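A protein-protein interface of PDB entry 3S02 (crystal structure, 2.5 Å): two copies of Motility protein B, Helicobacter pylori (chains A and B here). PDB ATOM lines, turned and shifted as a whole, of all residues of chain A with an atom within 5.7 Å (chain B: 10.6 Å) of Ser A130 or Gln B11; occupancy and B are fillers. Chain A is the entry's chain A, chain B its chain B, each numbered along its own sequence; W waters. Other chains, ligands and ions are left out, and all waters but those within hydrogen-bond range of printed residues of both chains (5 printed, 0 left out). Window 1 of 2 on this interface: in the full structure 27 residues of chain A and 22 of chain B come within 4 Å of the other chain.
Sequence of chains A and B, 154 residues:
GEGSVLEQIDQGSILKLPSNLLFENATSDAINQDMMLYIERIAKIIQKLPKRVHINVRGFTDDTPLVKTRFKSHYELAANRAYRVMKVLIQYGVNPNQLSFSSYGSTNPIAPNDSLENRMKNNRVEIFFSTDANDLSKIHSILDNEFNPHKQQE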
ATOM      1  N   GLN A  11       5.970  13.845  16.118  1.00  0.00           N
ATOM      2  CA  GLN A  11       4.620  14.303  16.415  1.00  0.00           C
ATOM      3  C   GLN A  11       3.806  14.755  15.182  1.00  0.00           C
ATOM      4  O   GLN A  11       2.744  15.318  15.321  1.00  0.00           O
ATOM      5  CB  GLN A  11       4.626  15.376  17.518  1.00  0.00           C
ATOM      6  CG  GLN A  11       5.135  14.872  18.944  1.00  0.00           C
ATOM      7  CD  GLN A  11       4.256  13.767  19.621  1.00  0.00           C
ATOM      8  OE1 GLN A  11       4.759  12.990  20.445  1.00  0.00           O
ATOM      9  NE2 GLN A  11       2.971  13.712  19.291  1.00  0.00           N
ATOM     10  N   GLY A  12       4.305  14.493  13.978  1.00  0.00           N
ATOM     11  CA  GLY A  12       3.503  14.712  12.799  1.00  0.00           C
ATOM     12  C   GLY A  12       4.278  14.734  11.493  1.00  0.00           C
ATOM     13  O   GLY A  12       5.471  14.464  11.470  1.00  0.00           O
ATOM     14  N   SER A  13       3.582  15.088  10.422  1.00  0.00           N
ATOM     15  CA  SER A  13       4.129  15.111   9.086  1.00  0.00           C
ATOM     16  C   SER A  13       4.213  16.574   8.569  1.00  0.00           C
ATOM     17  O   SER A  13       3.381  17.425   8.933  1.00  0.00           O
ATOM     18  CB  SER A  13       3.240  14.272   8.166  1.00  0.00           C
ATOM     19  OG  SER A  13       3.327  12.883   8.447  1.00  0.00           O
ATOM     20  N   ARG A  52      -9.319  12.957  13.398  1.00  0.00           N
ATOM     21  CA  ARG A  52      -8.745  13.833  14.412  1.00  0.00           C
ATOM     22  C   ARG A  52      -7.521  14.643  13.956  1.00  0.00           C
ATOM     23  O   ARG A  52      -6.961  15.424  14.737  1.00  0.00           O
ATOM     24  CB  ARG A  52      -8.423  13.019  15.655  1.00  0.00           C
ATOM     25  CG  ARG A  52      -9.613  12.190  16.190  1.00  0.00           C
ATOM     26  CD  ARG A  52      -9.124  10.851  16.737  1.00  0.00           C
ATOM     27  NE  ARG A  52      -8.563   9.972  15.700  1.00  0.00           N
ATOM     28  CZ  ARG A  52      -9.210   8.954  15.120  1.00  0.00           C
ATOM     29  NH1 ARG A  52     -10.481   8.686  15.441  1.00  0.00           N
ATOM     30  NH2 ARG A  52      -8.592   8.195  14.207  1.00  0.00           N
ATOM     31  N   VAL A  53      -7.134  14.491  12.691  1.00  0.00           N
ATOM     32  CA  VAL A  53      -6.025  15.251  12.142  1.00  0.00           C
ATOM     33  C   VAL A  53      -6.280  16.765  12.254  1.00  0.00           C
ATOM     34  O   VAL A  53      -7.395  17.228  12.027  1.00  0.00           O
ATOM     35  CB  VAL A  53      -5.720  14.833  10.693  1.00  0.00           C
ATOM     36  CG1 VAL A  53      -6.739  15.415   9.735  1.00  0.00           C
ATOM     37  CG2 VAL A  53      -4.364  15.286  10.302  1.00  0.00           C
ATOM     38  N   HIS A  54      -5.258  17.505  12.673  1.00  0.00           N
ATOM     39  CA  HIS A  54      -5.254  18.976  12.546  1.00  0.00           C
ATOM     40  C   HIS A  54      -4.159  19.421  11.572  1.00  0.00           C
ATOM     41  O   HIS A  54      -3.092  18.831  11.522  1.00  0.00           O
ATOM     42  CB  HIS A  54      -5.142  19.744  13.892  1.00  0.00           C
ATOM     43  CG  HIS A  54      -5.103  21.244  13.715  1.00  0.00           C
ATOM     44  ND1 HIS A  54      -6.242  22.034  13.732  1.00  0.00           N
ATOM     45  CD2 HIS A  54      -4.066  22.090  13.454  1.00  0.00           C
ATOM     46  CE1 HIS A  54      -5.901  23.295  13.508  1.00  0.00           C
ATOM     47  NE2 HIS A  54      -4.592  23.354  13.324  1.00  0.00           N
ATOM     48  N   ILE A  55      -4.462  20.455  10.797  1.00  0.00           N
ATOM     49  CA  ILE A  55      -3.583  20.955   9.764  1.00  0.00           C
ATOM     50  C   ILE A  55      -3.237  22.413  10.034  1.00  0.00           C
ATOM     51  O   ILE A  55      -4.099  23.310  10.040  1.00  0.00           O
ATOM     52  CB  ILE A  55      -4.188  20.797   8.362  1.00  0.00           C
ATOM     53  CG1 ILE A  55      -4.454  19.314   8.059  1.00  0.00           C
ATOM     54  CG2 ILE A  55      -3.252  21.357   7.307  1.00  0.00           C
ATOM     55  CD1 ILE A  55      -5.921  18.946   8.244  1.00  0.00           C
ATOM     56  N   PHE A 128       1.764  21.243   8.313  1.00  0.00           N
ATOM     57  CA  PHE A 128       2.120  20.345   9.395  1.00  0.00           C
ATOM     58  C   PHE A 128       0.851  19.649   9.856  1.00  0.00           C
ATOM     59  O   PHE A 128      -0.131  20.323  10.230  1.00  0.00           O
ATOM     60  CB  PHE A 128       2.814  21.076  10.545  1.00  0.00           C
ATOM     61  CG  PHE A 128       3.145  20.181  11.727  1.00  0.00           C
ATOM     62  CD1 PHE A 128       4.243  19.340  11.704  1.00  0.00           C
ATOM     63  CD2 PHE A 128       2.357  20.193  12.882  1.00  0.00           C
ATOM     64  CE1 PHE A 128       4.527  18.490  12.812  1.00  0.00           C
ATOM     65  CE2 PHE A 128       2.647  19.371  13.988  1.00  0.00           C
ATOM     66  CZ  PHE A 128       3.726  18.522  13.950  1.00  0.00           C
ATOM     67  N   PHE A 129       0.875  18.313   9.784  1.00  0.00           N
ATOM     68  CA  PHE A 129      -0.234  17.437  10.105  1.00  0.00           C
ATOM     69  C   PHE A 129       0.032  16.775  11.456  1.00  0.00           C
ATOM     70  O   PHE A 129       1.029  16.039  11.593  1.00  0.00           O
ATOM     71  CB  PHE A 129      -0.297  16.299   9.074  1.00  0.00           C
ATOM     72  CG  PHE A 129      -0.508  16.758   7.636  1.00  0.00           C
ATOM     73  CD1 PHE A 129      -1.742  16.599   7.023  1.00  0.00           C
ATOM     74  CD2 PHE A 129       0.548  17.312   6.896  1.00  0.00           C
ATOM     75  CE1 PHE A 129      -1.940  16.997   5.706  1.00  0.00           C
ATOM     76  CE2 PHE A 129       0.374  17.693   5.587  1.00  0.00           C
ATOM     77  CZ  PHE A 129      -0.864  17.538   4.971  1.00  0.00           C
ATOM     78  N   SER A 130      -0.871  16.955  12.427  1.00  0.00           N
ATOM     79  CA  SER A 130      -0.733  16.299  13.727  1.00  0.00           C
ATOM     80  C   SER A 130      -2.089  15.901  14.262  1.00  0.00           C
ATOM     81  O   SER A 130      -3.080  15.961  13.543  1.00  0.00           O
ATOM     82  CB  SER A 130      -0.059  17.253  14.723  1.00  0.00           C
ATOM     83  OG  SER A 130      -0.865  18.435  14.949  1.00  0.00           O
ATOM     84  N   THR A 131      -2.147  15.471  15.521  1.00  0.00           N
ATOM     85  CA  THR A 131      -3.444  15.364  16.176  1.00  0.00           C
ATOM     86  C   THR A 131      -3.365  15.803  17.610  1.00  0.00           C
ATOM     87  O   THR A 131      -2.286  15.945  18.144  1.00  0.00           O
ATOM     88  CB  THR A 131      -4.113  13.961  16.110  1.00  0.00           C
ATOM     89  OG1 THR A 131      -3.706  13.190  17.238  1.00  0.00           O
ATOM     90  CG2 THR A 131      -3.850  13.223  14.787  1.00  0.00           C
ATOM     91  N   ASP A 132      -4.532  15.965  18.225  1.00  0.00           N
ATOM     92  CA  ASP A 132      -4.668  16.482  19.578  1.00  0.00           C
ATOM     93  C   ASP A 132      -4.724  15.371  20.612  1.00  0.00           C
ATOM     94  O   ASP A 132      -5.132  15.616  21.752  1.00  0.00           O
ATOM     95  CB  ASP A 132      -5.928  17.353  19.685  1.00  0.00           C
ATOM     96  CG  ASP A 132      -7.185  16.673  19.106  1.00  0.00           C
ATOM     97  OD1 ASP A 132      -7.091  15.722  18.284  1.00  0.00           O
ATOM     98  OD2 ASP A 132      -8.292  17.108  19.474  1.00  0.00           O
ATOM     99  N   ALA A 133      -4.326  14.157  20.221  1.00  0.00           N
ATOM    100  CA  ALA A 133      -4.369  12.977  21.119  1.00  0.00           C
ATOM    101  C   ALA A 133      -4.018  13.334  22.574  1.00  0.00           C
ATOM    102  O   ALA A 133      -3.033  14.047  22.831  1.00  0.00           O
ATOM    103  CB  ALA A 133      -3.404  11.900  20.618  1.00  0.00           C
ATOM    104  N   GLU B   7      -2.796  22.709  30.561  1.00  0.00           N
ATOM    105  CA  GLU B   7      -3.371  21.459  30.102  1.00  0.00           C
ATOM    106  C   GLU B   7      -2.319  20.676  29.334  1.00  0.00           C
ATOM    107  O   GLU B   7      -1.502  21.251  28.609  1.00  0.00           O
ATOM    108  CB  GLU B   7      -4.580  21.723  29.222  1.00  0.00           C
ATOM    109  CG  GLU B   7      -5.458  20.504  29.016  1.00  0.00           C
ATOM    110  CD  GLU B   7      -6.486  20.703  27.899  1.00  0.00           C
ATOM    111  OE1 GLU B   7      -7.104  21.811  27.848  1.00  0.00           O
ATOM    112  OE2 GLU B   7      -6.664  19.745  27.086  1.00  0.00           O
ATOM    113  N   GLN B   8      -2.315  19.365  29.505  1.00  0.00           N
ATOM    114  CA  GLN B   8      -1.345  18.530  28.802  1.00  0.00           C
ATOM    115  C   GLN B   8      -2.052  17.839  27.666  1.00  0.00           C
ATOM    116  O   GLN B   8      -3.186  17.438  27.805  1.00  0.00           O
ATOM    117  CB  GLN B   8      -0.721  17.520  29.754  1.00  0.00           C
ATOM    118  CG  GLN B   8       0.547  16.894  29.242  1.00  0.00           C
ATOM    119  CD  GLN B   8       1.144  15.900  30.232  1.00  0.00           C
ATOM    120  OE1 GLN B   8       0.472  15.415  31.157  1.00  0.00           O
ATOM    121  NE2 GLN B   8       2.421  15.594  30.046  1.00  0.00           N
ATOM    122  N   ILE B   9      -1.416  17.757  26.516  1.00  0.00           N
ATOM    123  CA  ILE B   9      -1.861  16.795  25.502  1.00  0.00           C
ATOM    124  C   ILE B   9      -0.625  15.988  25.199  1.00  0.00           C
ATOM    125  O   ILE B   9       0.461  16.314  25.698  1.00  0.00           O
ATOM    126  CB  ILE B   9      -2.468  17.437  24.255  1.00  0.00           C
ATOM    127  CG1 ILE B   9      -1.513  18.485  23.670  1.00  0.00           C
ATOM    128  CG2 ILE B   9      -3.851  18.065  24.584  1.00  0.00           C
ATOM    129  CD1 ILE B   9      -1.813  18.880  22.254  1.00  0.00           C
ATOM    130  N   ASP B  10      -0.771  14.910  24.443  1.00  0.00           N
ATOM    131  CA  ASP B  10       0.339  13.967  24.292  1.00  0.00           C
ATOM    132  C   ASP B  10       1.504  14.547  23.533  1.00  0.00           C
ATOM    133  O   ASP B  10       2.632  14.111  23.760  1.00  0.00           O
ATOM    134  CB  ASP B  10      -0.125  12.631  23.704  1.00  0.00           C
ATOM    135  CG  ASP B  10      -1.153  11.911  24.624  1.00  0.00           C
ATOM    136  OD1 ASP B  10      -1.437  12.399  25.778  1.00  0.00           O
ATOM    137  OD2 ASP B  10      -1.654  10.854  24.179  1.00  0.00           O
ATOM    138  N   GLN B  11       1.262  15.538  22.656  1.00  0.00           N
ATOM    139  CA  GLN B  11       2.412  16.230  21.997  1.00  0.00           C
ATOM    140  C   GLN B  11       3.012  17.467  22.719  1.00  0.00           C
ATOM    141  O   GLN B  11       3.971  18.055  22.216  1.00  0.00           O
ATOM    142  CB  GLN B  11       2.173  16.525  20.499  1.00  0.00           C
ATOM    143  CG  GLN B  11       0.996  17.454  20.171  1.00  0.00           C
ATOM    144  CD  GLN B  11       0.968  17.957  18.695  1.00  0.00           C
ATOM    145  OE1 GLN B  11       1.956  18.462  18.151  1.00  0.00           O
ATOM    146  NE2 GLN B  11      -0.203  17.863  18.081  1.00  0.00           N
ATOM    147  N   GLY B  12       2.490  17.845  23.887  1.00  0.00           N
ATOM    148  CA  GLY B  12       3.001  19.051  24.541  1.00  0.00           C
ATOM    149  C   GLY B  12       2.115  19.669  25.601  1.00  0.00           C
ATOM    150  O   GLY B  12       1.167  19.048  26.073  1.00  0.00           O
ATOM    151  N   SER B  13       2.425  20.905  25.967  1.00  0.00           N
ATOM    152  CA  SER B  13       1.767  21.585  27.087  1.00  0.00           C
ATOM    153  C   SER B  13       1.114  22.843  26.564  1.00  0.00           C
ATOM    154  O   SER B  13       1.648  23.531  25.645  1.00  0.00           O
ATOM    155  CB  SER B  13       2.776  21.964  28.166  1.00  0.00           C
ATOM    156  OG  SER B  13       3.312  20.820  28.809  1.00  0.00           O
ATOM    157  N   ILE B  14      -0.060  23.111  27.130  1.00  0.00           N
ATOM    158  CA  ILE B  14      -0.866  24.256  26.790  1.00  0.00           C
ATOM    159  C   ILE B  14      -1.058  25.177  27.990  1.00  0.00           C
ATOM    160  O   ILE B  14      -1.724  24.819  28.962  1.00  0.00           O
ATOM    161  CB  ILE B  14      -2.254  23.815  26.297  1.00  0.00           C
ATOM    162  CG1 ILE B  14      -2.093  22.901  25.080  1.00  0.00           C
ATOM    163  CG2 ILE B  14      -3.128  25.079  25.970  1.00  0.00           C
ATOM    164  CD1 ILE B  14      -3.379  22.155  24.670  1.00  0.00           C
ATOM    165  N   ARG B  52      15.683  23.604  22.860  1.00  0.00           N
ATOM    166  CA  ARG B  52      15.015  22.790  21.824  1.00  0.00           C
ATOM    167  C   ARG B  52      13.492  22.862  21.932  1.00  0.00           C
ATOM    168  O   ARG B  52      12.781  22.224  21.147  1.00  0.00           O
ATOM    169  CB  ARG B  52      15.492  21.320  21.799  1.00  0.00           C
ATOM    170  CG  ARG B  52      14.987  20.426  22.959  1.00  0.00           C
ATOM    171  CD  ARG B  52      15.894  19.221  23.190  1.00  0.00           C
ATOM    172  NE  ARG B  52      15.828  18.801  24.590  1.00  0.00           N
ATOM    173  CZ  ARG B  52      16.618  19.258  25.574  1.00  0.00           C
ATOM    174  NH1 ARG B  52      17.566  20.158  25.317  1.00  0.00           N
ATOM    175  NH2 ARG B  52      16.458  18.821  26.825  1.00  0.00           N
ATOM    176  N   VAL B  53      13.006  23.619  22.907  1.00  0.00           N
ATOM    177  CA  VAL B  53      11.586  23.776  23.114  1.00  0.00           C
ATOM    178  C   VAL B  53      11.085  24.867  22.181  1.00  0.00           C
ATOM    179  O   VAL B  53      11.708  25.923  22.077  1.00  0.00           O
ATOM    180  CB  VAL B  53      11.265  24.126  24.577  1.00  0.00           C
ATOM    181  CG1 VAL B  53       9.795  24.292  24.770  1.00  0.00           C
ATOM    182  CG2 VAL B  53      11.775  23.011  25.489  1.00  0.00           C
ATOM    183  N   HIS B  54       9.982  24.605  21.490  1.00  0.00           N
ATOM    184  CA  HIS B  54       9.373  25.619  20.638  1.00  0.00           C
ATOM    185  C   HIS B  54       8.116  26.168  21.312  1.00  0.00           C
ATOM    186  O   HIS B  54       7.365  25.435  21.975  1.00  0.00           O
ATOM    187  CB  HIS B  54       9.130  25.103  19.197  1.00  0.00           C
ATOM    188  CG  HIS B  54      10.397  24.707  18.471  1.00  0.00           C
ATOM    189  ND1 HIS B  54      11.466  25.575  18.282  1.00  0.00           N
ATOM    190  CD2 HIS B  54      10.769  23.532  17.898  1.00  0.00           C
ATOM    191  CE1 HIS B  54      12.431  24.950  17.629  1.00  0.00           C
ATOM    192  NE2 HIS B  54      12.033  23.710  17.381  1.00  0.00           N
ATOM    193  N   ILE B  55       7.925  27.474  21.166  1.00  0.00           N
ATOM    194  CA  ILE B  55       6.900  28.164  21.892  1.00  0.00           C
ATOM    195  C   ILE B  55       5.990  28.837  20.879  1.00  0.00           C
ATOM    196  O   ILE B  55       6.439  29.714  20.138  1.00  0.00           O
ATOM    197  CB  ILE B  55       7.534  29.163  22.917  1.00  0.00           C
ATOM    198  CG1 ILE B  55       8.544  28.441  23.829  1.00  0.00           C
ATOM    199  CG2 ILE B  55       6.479  29.915  23.753  1.00  0.00           C
ATOM    200  CD1 ILE B  55       9.597  29.402  24.471  1.00  0.00           C
ATOM    201  N   ASN B  56       4.719  28.426  20.847  1.00  0.00           N
ATOM    202  CA  ASN B  56       3.728  28.958  19.883  1.00  0.00           C
ATOM    203  C   ASN B  56       2.599  29.643  20.614  1.00  0.00           C
ATOM    204  O   ASN B  56       1.931  28.999  21.431  1.00  0.00           O
ATOM    205  CB  ASN B  56       3.116  27.834  19.043  1.00  0.00           C
ATOM    206  CG  ASN B  56       2.252  28.363  17.913  1.00  0.00           C
ATOM    207  OD1 ASN B  56       2.750  28.932  16.949  1.00  0.00           O
ATOM    208  ND2 ASN B  56       0.960  28.179  18.023  1.00  0.00           N
ATOM    209  N   ARG B  58      -1.059  31.208  20.367  1.00  0.00           N
ATOM    210  CA  ARG B  58      -2.188  30.972  19.407  1.00  0.00           C
ATOM    211  C   ARG B  58      -3.409  31.717  19.847  1.00  0.00           C
ATOM    212  O   ARG B  58      -3.680  31.795  21.042  1.00  0.00           O
ATOM    213  CB  ARG B  58      -2.475  29.469  19.273  1.00  0.00           C
ATOM    214  CG  ARG B  58      -2.272  28.813  20.602  1.00  0.00           C
ATOM    215  CD  ARG B  58      -2.052  27.347  20.601  1.00  0.00           C
ATOM    216  NE  ARG B  58      -1.116  26.836  19.620  1.00  0.00           N
ATOM    217  CZ  ARG B  58      -1.137  25.558  19.262  1.00  0.00           C
ATOM    218  NH1 ARG B  58      -2.031  24.737  19.831  1.00  0.00           N
ATOM    219  NH2 ARG B  58      -0.300  25.106  18.348  1.00  0.00           N
ATOM    220  N   TYR B 104      -6.576  30.645  14.923  1.00  0.00           N
ATOM    221  CA  TYR B 104      -7.694  29.712  14.593  1.00  0.00           C
ATOM    222  C   TYR B 104      -8.943  30.452  14.236  1.00  0.00           C
ATOM    223  O   TYR B 104      -9.952  29.833  13.937  1.00  0.00           O
ATOM    224  CB  TYR B 104      -8.036  28.769  15.749  1.00  0.00           C
ATOM    225  CG  TYR B 104      -6.909  27.827  16.097  1.00  0.00           C
ATOM    226  CD1 TYR B 104      -7.016  26.456  15.847  1.00  0.00           C
ATOM    227  CD2 TYR B 104      -5.720  28.310  16.683  1.00  0.00           C
ATOM    228  CE1 TYR B 104      -5.993  25.588  16.162  1.00  0.00           C
ATOM    229  CE2 TYR B 104      -4.673  27.431  16.988  1.00  0.00           C
ATOM    230  CZ  TYR B 104      -4.827  26.088  16.722  1.00  0.00           C
ATOM    231  OH  TYR B 104      -3.806  25.257  17.048  1.00  0.00           O
ATOM    232  N   ASN B 108     -12.778  25.967  15.868  1.00  0.00           N
ATOM    233  CA  ASN B 108     -12.420  25.290  17.122  1.00  0.00           C
ATOM    234  C   ASN B 108     -12.895  25.950  18.396  1.00  0.00           C
ATOM    235  O   ASN B 108     -12.088  26.149  19.321  1.00  0.00           O
ATOM    236  CB  ASN B 108     -10.906  25.062  17.218  1.00  0.00           C
ATOM    237  CG  ASN B 108     -10.500  23.810  16.517  1.00  0.00           C
ATOM    238  OD1 ASN B 108     -11.331  22.891  16.365  1.00  0.00           O
ATOM    239  ND2 ASN B 108      -9.248  23.750  16.048  1.00  0.00           N
ATOM    240  N   ILE B 127      -0.473  29.427  24.919  1.00  0.00           N
ATOM    241  CA  ILE B 127       0.878  29.166  24.515  1.00  0.00           C
ATOM    242  C   ILE B 127       1.066  27.661  24.562  1.00  0.00           C
ATOM    243  O   ILE B 127       0.830  27.003  25.591  1.00  0.00           O
ATOM    244  CB  ILE B 127       1.872  29.881  25.426  1.00  0.00           C
ATOM    245  CG1 ILE B 127       1.521  31.372  25.528  1.00  0.00           C
ATOM    246  CG2 ILE B 127       3.264  29.720  24.866  1.00  0.00           C
ATOM    247  CD1 ILE B 127       2.428  32.109  26.463  1.00  0.00           C
ATOM    248  N   PHE B 128       1.473  27.122  23.432  1.00  0.00           N
ATOM    249  CA  PHE B 128       1.724  25.720  23.298  1.00  0.00           C
ATOM    250  C   PHE B 128       3.218  25.477  23.285  1.00  0.00           C
ATOM    251  O   PHE B 128       3.957  26.146  22.548  1.00  0.00           O
ATOM    252  CB  PHE B 128       1.092  25.263  22.006  1.00  0.00           C
ATOM    253  CG  PHE B 128       1.323  23.831  21.690  1.00  0.00           C
ATOM    254  CD1 PHE B 128       0.758  22.824  22.483  1.00  0.00           C
ATOM    255  CD2 PHE B 128       2.034  23.475  20.546  1.00  0.00           C
ATOM    256  CE1 PHE B 128       0.955  21.494  22.189  1.00  0.00           C
ATOM    257  CE2 PHE B 128       2.220  22.120  20.235  1.00  0.00           C
ATOM    258  CZ  PHE B 128       1.676  21.135  21.073  1.00  0.00           C
ATOM    259  N   PHE B 129       3.657  24.517  24.095  1.00  0.00           N
ATOM    260  CA  PHE B 129       5.066  24.154  24.202  1.00  0.00           C
ATOM    261  C   PHE B 129       5.335  22.735  23.648  1.00  0.00           C
ATOM    262  O   PHE B 129       4.710  21.768  24.078  1.00  0.00           O
ATOM    263  CB  PHE B 129       5.483  24.188  25.673  1.00  0.00           C
ATOM    264  CG  PHE B 129       5.341  25.539  26.334  1.00  0.00           C
ATOM    265  CD1 PHE B 129       6.466  26.352  26.538  1.00  0.00           C
ATOM    266  CD2 PHE B 129       4.096  25.982  26.807  1.00  0.00           C
ATOM    267  CE1 PHE B 129       6.354  27.590  27.153  1.00  0.00           C
ATOM    268  CE2 PHE B 129       3.977  27.200  27.445  1.00  0.00           C
ATOM    269  CZ  PHE B 129       5.107  28.019  27.622  1.00  0.00           C
ATOM    270  N   SER B 130       6.292  22.590  22.747  1.00  0.00           N
ATOM    271  CA  SER B 130       6.575  21.282  22.159  1.00  0.00           C
ATOM    272  C   SER B 130       8.030  21.171  21.738  1.00  0.00           C
ATOM    273  O   SER B 130       8.831  22.057  22.016  1.00  0.00           O
ATOM    274  CB  SER B 130       5.685  21.051  20.946  1.00  0.00           C
ATOM    275  OG  SER B 130       5.993  22.045  19.979  1.00  0.00           O
ATOM    276  N   THR B 131       8.370  20.071  21.074  1.00  0.00           N
ATOM    277  CA  THR B 131       9.698  19.902  20.475  1.00  0.00           C
ATOM    278  C   THR B 131       9.592  19.270  19.072  1.00  0.00           C
ATOM    279  O   THR B 131       8.531  18.802  18.674  1.00  0.00           O
ATOM    280  CB  THR B 131      10.666  19.063  21.369  1.00  0.00           C
ATOM    281  OG1 THR B 131      10.357  17.670  21.256  1.00  0.00           O
ATOM    282  CG2 THR B 131      10.604  19.477  22.841  1.00  0.00           C
ATOM    283  N   ASP B 132      10.697  19.277  18.339  1.00  0.00           N
ATOM    284  CA  ASP B 132      10.815  18.677  17.014  1.00  0.00           C
ATOM    285  C   ASP B 132      11.536  17.331  17.018  1.00  0.00           C
ATOM    286  O   ASP B 132      12.132  16.952  16.001  1.00  0.00           O
ATOM    287  CB  ASP B 132      11.602  19.613  16.120  1.00  0.00           C
ATOM    288  CG  ASP B 132      10.762  20.775  15.614  1.00  0.00           C
ATOM    289  OD1 ASP B 132       9.499  20.739  15.728  1.00  0.00           O
ATOM    290  OD2 ASP B 132      11.387  21.733  15.084  1.00  0.00           O
ATOM    291  N   ALA B 133      11.510  16.631  18.151  1.00  0.00           N
ATOM    292  CA  ALA B 133      12.047  15.276  18.276  1.00  0.00           C
ATOM    293  C   ALA B 133      11.770  14.422  17.024  1.00  0.00           C
ATOM    294  O   ALA B 133      10.627  14.351  16.555  1.00  0.00           O
ATOM    295  CB  ALA B 133      11.454  14.607  19.508  1.00  0.00           C
HETATM  296  O   HOH W   1      -2.953  18.859  16.608  1.00  0.00           O
HETATM  297  O   HOH W   2       3.933  11.613  23.029  1.00  0.00           O
HETATM  298  O   HOH W   3       8.068  15.786  17.171  1.00  0.00           O
HETATM  299  O   HOH W   4       0.573  15.261  16.917  1.00  0.00           O
HETATM  300  O   HOH W   5      -1.204  15.290  21.086  1.00  0.00           O
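Ser A130 touches one residue of chain B. Of chain A, only Gln A11 (3.2 Å), Ser A130 (3.3 Å) and Thr A131 (2.8 Å) come within 4 Å of Gln B11. No residue of chain B comes within 4 Å of Val A53. Ala A133 touches just these residues of chain B: Ile B9 and Asp B10. Of the printed residues of chain A, Ile B9 touches Asp A132 and Ala A133. Printed residues of chain A within 4 Å of Tyr B104: His A54. Of the printed residues of chain A, Asp B10 touches Ala A133. Printed residues of chain B within 4 Å of His A54: Tyr B104. Phe B128 touches none of the printed residues of chain A. The nearest residue of chain B that does not touch Ser A130 is Phe B128 (7.1 Å). The nearest printed residue of chain A that does not touch Asp B10 is Gln A11 (4.1 Å).
The guanidinium group of Arg B58 sits at hydrogen-bond distance from the side-chain hydroxyl of Tyr B104, at 3.3 Å. N of His A54 lies within hydrogen-bond range of O of Ser A130. The side-chain hydroxyl of Thr A131 lies within hydrogen-bond range of the backbone NH of Ala A133.
Water W4 lies within hydrogen-bond range of O of Gln A11, NE2 of Gln B11 and N of Thr A131. Water W1 lies within hydrogen-bond range of OG of Ser A130, NE2 of Gln B11 and O of Thr A131. Water W5 lies within hydrogen-bond range of the backbone carbonyl oxygen (O) of Ala A133, the backbone NH (N) of Gln B11, the backbone carbonyl oxygen (O) of Thr A131 and the backbone NH (N) of Asp B10. Water W2 lies within hydrogen-bond range of O of Asp B10 (2.9 Å) and OE1 of Gln A11 (3.0 Å). Water W3 lies within hydrogen-bond range of O of Ala B133 (3.0 Å), N of Gln A11 (3.0 Å) and O of Thr B131 (3.4 Å).
The side-chain amide nitrogen (NE2) of Gln B11 is in hydrogen-bond range of the backbone carbonyl oxygen (O) of Thr A131, 2.8 Å away. The side-chain amide nitrogen of Gln B11 is in hydrogen-bond range of the side-chain hydroxyl of Ser A130, 3.3 Å away. The backbone NH (N) of Asp B10 lies within hydrogen-bond range of the backbone carbonyl oxygen (O) of Ala A133 (2.9 Å).
Gln B11 touches its own counterpart, Gln A11. Ser A130 touches Gln B11, but with the chains exchanged Gln A11 does not touch Ser B130 (6.5 Å). Thr A131 touches Gln B11, but with the chains exchanged Gln A11 does not touch Thr B131 (5.2 Å). Positions printed for both chains: 11, 12, 13, 52, 53, 54, 55, 128, 129, 130, 131, 132 and 133. Of the 7 pairs that touch across the chains among the printed residues, 1 has its exchanged pair printed and touching as well.
Gln B11 touches Gln A11. His A54 touches Tyr B104. O of Asp A132 touches CG2 of Ile B9, 3.96 Å away. CB of Ile B9 touches O of Ala A133, 3.7 Å away.
Of the 23 printed residues of chain B, 4 touch a printed residue of chain A. Hydrophobic or aromatic side chains of chain B that line the printed part of chain A: Ile B9 and Tyr B104. Printed residues of chain A that touch a printed residue of chain B: Gln A11, His A54, Ser A130, Thr A131, Asp A132 and Ala A133. Hydrophobic or aromatic side chains of chain A within 4 Å of the printed part of chain B: His A54. Among the printed residues, no Asp or Glu carboxylate lies within 4 Å of a Lys or Arg side-chain nitrogen of the other chain.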
